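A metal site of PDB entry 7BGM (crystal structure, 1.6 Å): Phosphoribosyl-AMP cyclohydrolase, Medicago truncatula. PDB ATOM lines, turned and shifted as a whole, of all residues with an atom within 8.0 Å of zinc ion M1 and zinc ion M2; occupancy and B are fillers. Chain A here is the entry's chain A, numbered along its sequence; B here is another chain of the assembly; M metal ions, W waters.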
ATOM      1  N   LEU A  32     -27.948 -15.873   0.960  1.00  0.00           N
ATOM      2  CA  LEU A  32     -28.045 -15.565  -0.455  1.00  0.00           C
ATOM      3  C   LEU A  32     -28.132 -14.068  -0.703  1.00  0.00           C
ATOM      4  O   LEU A  32     -27.485 -13.545  -1.633  1.00  0.00           O
ATOM      5  CB  LEU A  32     -29.297 -16.250  -1.035  1.00  0.00           C
ATOM      6  CG  LEU A  32     -29.337 -17.778  -0.819  1.00  0.00           C
ATOM      7  CD1 LEU A  32     -30.672 -18.403  -1.289  1.00  0.00           C
ATOM      8  CD2 LEU A  32     -28.145 -18.444  -1.510  1.00  0.00           C
ATOM      9  N   MET A  33     -28.998 -13.394   0.060  1.00  0.00           N
ATOM     10  CA  MET A  33     -29.256 -11.960  -0.145  1.00  0.00           C
ATOM     11  C   MET A  33     -30.070 -11.475   1.050  1.00  0.00           C
ATOM     12  O   MET A  33     -30.671 -12.281   1.774  1.00  0.00           O
ATOM     13  CB  MET A  33     -30.035 -11.657  -1.453  1.00  0.00           C
ATOM     14  CG  MET A  33     -31.426 -12.302  -1.449  1.00  0.00           C
ATOM     15  SD  MET A  33     -32.450 -11.845  -2.869  1.00  0.00           S
ATOM     16  CE  MET A  33     -32.861 -10.142  -2.477  1.00  0.00           C
ATOM     17  N   GLN A  34     -30.116 -10.152   1.211  1.00  0.00           N
ATOM     18  CA  GLN A  34     -30.937  -9.585   2.255  1.00  0.00           C
ATOM     19  C   GLN A  34     -31.627  -8.363   1.674  1.00  0.00           C
ATOM     20  O   GLN A  34     -31.001  -7.579   0.945  1.00  0.00           O
ATOM     21  CB  GLN A  34     -30.109  -9.214   3.506  1.00  0.00           C
ATOM     22  CG  GLN A  34     -30.902  -8.419   4.579  1.00  0.00           C
ATOM     23  CD  GLN A  34     -30.693  -6.894   4.472  1.00  0.00           C
ATOM     24  OE1 GLN A  34     -29.565  -6.403   4.546  1.00  0.00           O
ATOM     25  NE2 GLN A  34     -31.779  -6.156   4.294  1.00  0.00           N
ATOM     26  N   TRP A  62     -41.220  -7.102  -5.560  1.00  0.00           N
ATOM     27  CA  TRP A  62     -40.530  -7.848  -6.598  1.00  0.00           C
ATOM     28  C   TRP A  62     -40.155  -9.217  -6.066  1.00  0.00           C
ATOM     29  O   TRP A  62     -39.867  -9.399  -4.881  1.00  0.00           O
ATOM     30  CB  TRP A  62     -39.276  -7.136  -7.132  1.00  0.00           C
ATOM     31  CG  TRP A  62     -38.145  -7.020  -6.146  1.00  0.00           C
ATOM     32  CD1 TRP A  62     -38.052  -6.159  -5.058  1.00  0.00           C
ATOM     33  CD2 TRP A  62     -36.912  -7.743  -6.191  1.00  0.00           C
ATOM     34  NE1 TRP A  62     -36.824  -6.336  -4.423  1.00  0.00           N
ATOM     35  CE2 TRP A  62     -36.110  -7.287  -5.109  1.00  0.00           C
ATOM     36  CE3 TRP A  62     -36.396  -8.708  -7.064  1.00  0.00           C
ATOM     37  CZ2 TRP A  62     -34.822  -7.799  -4.857  1.00  0.00           C
ATOM     38  CZ3 TRP A  62     -35.118  -9.202  -6.834  1.00  0.00           C
ATOM     39  CH2 TRP A  62     -34.349  -8.763  -5.714  1.00  0.00           C
ATOM     40  N   LYS A  64     -37.602 -12.349  -6.376  1.00  0.00           N
ATOM     41  CA  LYS A  64     -36.277 -12.709  -6.854  1.00  0.00           C
ATOM     42  C   LYS A  64     -36.405 -13.777  -7.927  1.00  0.00           C
ATOM     43  O   LYS A  64     -37.073 -14.804  -7.723  1.00  0.00           O
ATOM     44  CB  LYS A  64     -35.436 -13.195  -5.684  1.00  0.00           C
ATOM     45  CG  LYS A  64     -34.150 -13.808  -6.091  1.00  0.00           C
ATOM     46  CD  LYS A  64     -33.235 -12.743  -6.703  1.00  0.00           C
ATOM     47  CE  LYS A  64     -32.416 -13.279  -7.829  1.00  0.00           C
ATOM     48  NZ  LYS A  64     -31.544 -12.166  -8.374  1.00  0.00           N
ATOM     49  N   THR A  96     -27.809 -16.030  -7.068  1.00  0.00           N
ATOM     50  CA  THR A  96     -28.795 -15.085  -6.574  1.00  0.00           C
ATOM     51  C   THR A  96     -28.461 -13.647  -6.953  1.00  0.00           C
ATOM     52  O   THR A  96     -29.370 -12.831  -7.125  1.00  0.00           O
ATOM     53  CB  THR A  96     -28.887 -15.228  -5.039  1.00  0.00           C
ATOM     54  OG1 THR A  96     -29.381 -16.546  -4.711  1.00  0.00           O
ATOM     55  CG2 THR A  96     -29.791 -14.149  -4.425  1.00  0.00           C
ATOM     56  N   CYS A  97     -27.174 -13.315  -7.095  1.00  0.00           N
ATOM     57  CA  CYS A  97     -26.809 -11.914  -7.295  1.00  0.00           C
ATOM     58  C   CYS A  97     -26.933 -11.520  -8.771  1.00  0.00           C
ATOM     59  O   CYS A  97     -26.627 -12.310  -9.672  1.00  0.00           O
ATOM     60  CB  CYS A  97     -25.382 -11.623  -6.762  1.00  0.00           C
ATOM     61  SG  CYS A  97     -25.024  -9.831  -6.776  1.00  0.00           S
ATOM     62  N   HIS A  98     -27.437 -10.311  -9.012  1.00  0.00           N
ATOM     63  CA  HIS A  98     -27.524  -9.773 -10.362  1.00  0.00           C
ATOM     64  C   HIS A  98     -26.172  -9.709 -11.048  1.00  0.00           C
ATOM     65  O   HIS A  98     -26.104  -9.674 -12.285  1.00  0.00           O
ATOM     66  CB  HIS A  98     -28.150  -8.375 -10.345  1.00  0.00           C
ATOM     67  CG  HIS A  98     -27.300  -7.342  -9.653  1.00  0.00           C
ATOM     68  ND1 HIS A  98     -26.431  -6.513 -10.324  1.00  0.00           N
ATOM     69  CD2 HIS A  98     -27.200  -7.011  -8.341  1.00  0.00           C
ATOM     70  CE1 HIS A  98     -25.819  -5.719  -9.461  1.00  0.00           C
ATOM     71  NE2 HIS A  98     -26.267  -5.991  -8.248  1.00  0.00           N
ATOM     72  N   THR A  99     -25.086  -9.664 -10.276  1.00  0.00           N
ATOM     73  CA  THR A  99     -23.746  -9.649 -10.856  1.00  0.00           C
ATOM     74  C   THR A  99     -23.342 -11.011 -11.396  1.00  0.00           C
ATOM     75  O   THR A  99     -22.304 -11.116 -12.059  1.00  0.00           O
ATOM     76  CB  THR A  99     -22.695  -9.236  -9.816  1.00  0.00           C
ATOM     77  OG1 THR A  99     -22.645 -10.212  -8.763  1.00  0.00           O
ATOM     78  CG2 THR A  99     -22.991  -7.863  -9.232  1.00  0.00           C
ATOM     79  N   GLY A 100     -24.115 -12.067 -11.119  1.00  0.00           N
ATOM     80  CA  GLY A 100     -23.751 -13.424 -11.478  1.00  0.00           C
ATOM     81  C   GLY A 100     -23.128 -14.233 -10.350  1.00  0.00           C
ATOM     82  O   GLY A 100     -23.046 -15.471 -10.472  1.00  0.00           O
ATOM     83  N   ALA A 101     -22.707 -13.577  -9.271  1.00  0.00           N
ATOM     84  CA  ALA A 101     -22.164 -14.281  -8.112  1.00  0.00           C
ATOM     85  C   ALA A 101     -23.224 -15.162  -7.469  1.00  0.00           C
ATOM     86  O   ALA A 101     -24.414 -14.866  -7.515  1.00  0.00           O
ATOM     87  CB  ALA A 101     -21.658 -13.280  -7.069  1.00  0.00           C
ATOM     88  N   GLU A 102     -22.783 -16.250  -6.840  1.00  0.00           N
ATOM     89  CA  GLU A 102     -23.718 -17.215  -6.293  1.00  0.00           C
ATOM     90  C   GLU A 102     -24.586 -16.615  -5.186  1.00  0.00           C
ATOM     91  O   GLU A 102     -25.772 -16.941  -5.057  1.00  0.00           O
ATOM     92  CB  GLU A 102     -22.926 -18.420  -5.789  1.00  0.00           C
ATOM     93  CG  GLU A 102     -23.734 -19.572  -5.488  1.00  0.00           C
ATOM     94  CD  GLU A 102     -22.870 -20.804  -5.417  1.00  0.00           C
ATOM     95  OE1 GLU A 102     -22.205 -21.125  -6.423  1.00  0.00           O
ATOM     96  OE2 GLU A 102     -22.816 -21.397  -4.350  1.00  0.00           O
ATOM     97  N   THR A 103     -23.986 -15.728  -4.398  1.00  0.00           N
ATOM     98  CA  THR A 103     -24.676 -14.938  -3.384  1.00  0.00           C
ATOM     99  C   THR A 103     -24.261 -13.500  -3.547  1.00  0.00           C
ATOM    100  O   THR A 103     -23.286 -13.178  -4.256  1.00  0.00           O
ATOM    101  CB  THR A 103     -24.335 -15.347  -1.936  1.00  0.00           C
ATOM    102  OG1 THR A 103     -23.007 -14.863  -1.635  1.00  0.00           O
ATOM    103  CG2 THR A 103     -24.413 -16.895  -1.772  1.00  0.00           C
ATOM    104  N   CYS A 104     -24.978 -12.651  -2.848  1.00  0.00           N
ATOM    105  CA  CYS A 104     -24.647 -11.232  -2.916  1.00  0.00           C
ATOM    106  C   CYS A 104     -23.427 -10.849  -2.045  1.00  0.00           C
ATOM    107  O   CYS A 104     -23.006  -9.686  -2.080  1.00  0.00           O
ATOM    108  CB  CYS A 104     -25.850 -10.375  -2.511  1.00  0.00           C
ATOM    109  SG  CYS A 104     -27.242 -10.435  -3.652  1.00  0.00           S
ATOM    110  N   TYR A 105     -22.832 -11.780  -1.318  1.00  0.00           N
ATOM    111  CA  TYR A 105     -21.802 -11.468  -0.304  1.00  0.00           C
ATOM    112  C   TYR A 105     -20.474 -12.039  -0.742  1.00  0.00           C
ATOM    113  O   TYR A 105     -20.197 -13.228  -0.530  1.00  0.00           O
ATOM    114  CB  TYR A 105     -22.200 -11.981   1.092  1.00  0.00           C
ATOM    115  CG  TYR A 105     -23.460 -11.340   1.644  1.00  0.00           C
ATOM    116  CD1 TYR A 105     -23.383 -10.179   2.442  1.00  0.00           C
ATOM    117  CD2 TYR A 105     -24.735 -11.842   1.327  1.00  0.00           C
ATOM    118  CE1 TYR A 105     -24.536  -9.597   2.960  1.00  0.00           C
ATOM    119  CE2 TYR A 105     -25.893 -11.252   1.823  1.00  0.00           C
ATOM    120  CZ  TYR A 105     -25.785 -10.131   2.648  1.00  0.00           C
ATOM    121  OH  TYR A 105     -26.958  -9.571   3.132  1.00  0.00           O
ATOM    122  N   TYR A 106     -19.678 -11.201  -1.396  1.00  0.00           N
ATOM    123  CA  TYR A 106     -18.377 -11.574  -1.940  1.00  0.00           C
ATOM    124  C   TYR A 106     -17.340 -10.456  -1.758  1.00  0.00           C
ATOM    125  O   TYR A 106     -16.287 -10.464  -2.430  1.00  0.00           O
ATOM    126  CB  TYR A 106     -18.530 -11.923  -3.428  1.00  0.00           C
ATOM    127  CG  TYR A 106     -19.259 -10.882  -4.197  1.00  0.00           C
ATOM    128  CD1 TYR A 106     -18.589  -9.734  -4.639  1.00  0.00           C
ATOM    129  CD2 TYR A 106     -20.604 -11.038  -4.534  1.00  0.00           C
ATOM    130  CE1 TYR A 106     -19.234  -8.762  -5.356  1.00  0.00           C
ATOM    131  CE2 TYR A 106     -21.287 -10.062  -5.253  1.00  0.00           C
ATOM    132  CZ  TYR A 106     -20.590  -8.923  -5.665  1.00  0.00           C
ATOM    133  OH  TYR A 106     -21.200  -7.910  -6.372  1.00  0.00           O
ATOM    134  N   LYS B  12     -22.942   2.024   1.817  1.00  0.00           N
ATOM    135  CA  LYS B  12     -24.173   2.743   1.504  1.00  0.00           C
ATOM    136  C   LYS B  12     -25.034   2.801   2.769  1.00  0.00           C
ATOM    137  O   LYS B  12     -25.971   2.020   2.966  1.00  0.00           O
ATOM    138  CB  LYS B  12     -24.896   2.057   0.346  1.00  0.00           C
ATOM    139  CG  LYS B  12     -26.186   2.721  -0.118  1.00  0.00           C
ATOM    140  CD  LYS B  12     -26.711   2.065  -1.390  1.00  0.00           C
ATOM    141  CE  LYS B  12     -28.241   2.000  -1.435  1.00  0.00           C
ATOM    142  NZ  LYS B  12     -28.712   0.574  -1.551  1.00  0.00           N
ATOM    143  N   ASP B  80     -22.468  -6.819   1.127  1.00  0.00           N
ATOM    144  CA  ASP B  80     -23.200  -7.308  -0.043  1.00  0.00           C
ATOM    145  C   ASP B  80     -22.927  -6.430  -1.260  1.00  0.00           C
ATOM    146  O   ASP B  80     -22.203  -5.426  -1.196  1.00  0.00           O
ATOM    147  CB  ASP B  80     -24.689  -7.503   0.274  1.00  0.00           C
ATOM    148  CG  ASP B  80     -25.520  -6.243   0.231  1.00  0.00           C
ATOM    149  OD1 ASP B  80     -24.906  -5.168   0.450  1.00  0.00           O
ATOM    150  OD2 ASP B  80     -26.798  -6.364   0.024  1.00  0.00           O
ATOM    151  N   CYS B  81     -23.493  -6.835  -2.406  1.00  0.00           N
ATOM    152  CA  CYS B  81     -23.105  -6.248  -3.706  1.00  0.00           C
ATOM    153  C   CYS B  81     -23.356  -4.740  -3.776  1.00  0.00           C
ATOM    154  O   CYS B  81     -22.592  -4.009  -4.428  1.00  0.00           O
ATOM    155  CB  CYS B  81     -23.882  -6.960  -4.824  1.00  0.00           C
ATOM    156  SG  CYS B  81     -25.704  -6.889  -4.630  1.00  0.00           S
ATOM    157  N   ASP B  82     -24.446  -4.249  -3.163  1.00  0.00           N
ATOM    158  CA  ASP B  82     -24.710  -2.803  -3.162  1.00  0.00           C
ATOM    159  C   ASP B  82     -24.308  -2.119  -1.867  1.00  0.00           C
ATOM    160  O   ASP B  82     -24.562  -0.900  -1.696  1.00  0.00           O
ATOM    161  CB  ASP B  82     -26.183  -2.498  -3.521  1.00  0.00           C
ATOM    162  CG  ASP B  82     -27.193  -3.170  -2.594  1.00  0.00           C
ATOM    163  OD1 ASP B  82     -26.816  -3.859  -1.615  1.00  0.00           O
ATOM    164  OD2 ASP B  82     -28.415  -2.995  -2.879  1.00  0.00           O
ATOM    165  N   ARG B  83     -23.623  -2.856  -0.974  1.00  0.00           N
ATOM    166  CA  ARG B  83     -22.863  -2.297   0.164  1.00  0.00           C
ATOM    167  C   ARG B  83     -23.757  -1.699   1.251  1.00  0.00           C
ATOM    168  O   ARG B  83     -23.323  -0.807   1.998  1.00  0.00           O
ATOM    169  CB  ARG B  83     -21.813  -1.273  -0.327  1.00  0.00           C
ATOM    170  CG  ARG B  83     -21.027  -1.739  -1.562  1.00  0.00           C
ATOM    171  CD  ARG B  83     -20.043  -0.715  -2.069  1.00  0.00           C
ATOM    172  NE  ARG B  83     -18.833  -0.685  -1.284  1.00  0.00           N
ATOM    173  CZ  ARG B  83     -17.790  -1.507  -1.441  1.00  0.00           C
ATOM    174  NH1 ARG B  83     -17.813  -2.519  -2.334  1.00  0.00           N
ATOM    175  NH2 ARG B  83     -16.714  -1.333  -0.684  1.00  0.00           N
ATOM    176  N   ASP B  84     -24.991  -2.194   1.407  1.00  0.00           N
ATOM    177  CA  ASP B  84     -25.852  -1.757   2.521  1.00  0.00           C
ATOM    178  C   ASP B  84     -26.126  -2.864   3.524  1.00  0.00           C
ATOM    179  O   ASP B  84     -26.945  -2.678   4.436  1.00  0.00           O
ATOM    180  CB  ASP B  84     -27.186  -1.173   2.004  1.00  0.00           C
ATOM    181  CG  ASP B  84     -27.937  -2.136   1.156  1.00  0.00           C
ATOM    182  OD1 ASP B  84     -27.503  -3.296   1.107  1.00  0.00           O
ATOM    183  OD2 ASP B  84     -28.925  -1.761   0.496  1.00  0.00           O
HETATM  184 ZN    ZN M   1     -26.476  -8.979  -5.273  1.00  0.00          ZN
HETATM  185 ZN    ZN M   2     -26.129  -5.151  -6.409  1.00  0.00          ZN
HETATM  186 ZN    ZN M   3     -27.917  -4.770  -0.211  1.00  0.00          ZN
HETATM  187  O   HOH W   1     -27.741  -3.783  -5.950  1.00  0.00           O
HETATM  188  O   HOH W   2     -23.954  -3.932  -6.989  1.00  0.00           O
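The nearest printed residue that does not touch zinc ion M1 is Thr 96 (5.2 Å).
Zinc ion M1 is bound by the side-chain sulfur (SG) of Cys 97, the side-chain sulfur (SG) of Cys 104 and the side-chain sulfur (SG) of Cys 81 of chain B.
Zinc ion M2 is bound by NE2 of His 98 (2.0 Å), water W1 (2.2 Å), SG of Cys 81 of chain B (2.5 Å) and water W2 (2.6 Å).
Merely in contact with zinc ion M2: Asp 82 of chain B. Within 4 Å of zinc ion M2: His 98, Cys 81 of chain B and Asp 82 of chain B. The nearest printed residue that does not touch zinc ion M2 is Cys 97 (4.8 Å).
The side-chain hydroxyl (OG1) of Thr 99 sits close to the side-chain sulfur (SG) of Cys 97 (3.1 Å). N of Cys 104 sits at hydrogen-bond distance from O of Leu 32 (2.9 Å). The side-chain amino group of Lys 12 of chain B is in salt-bridge range of the side-chain carboxylate of Asp 82 of chain B, 3.8 Å away.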
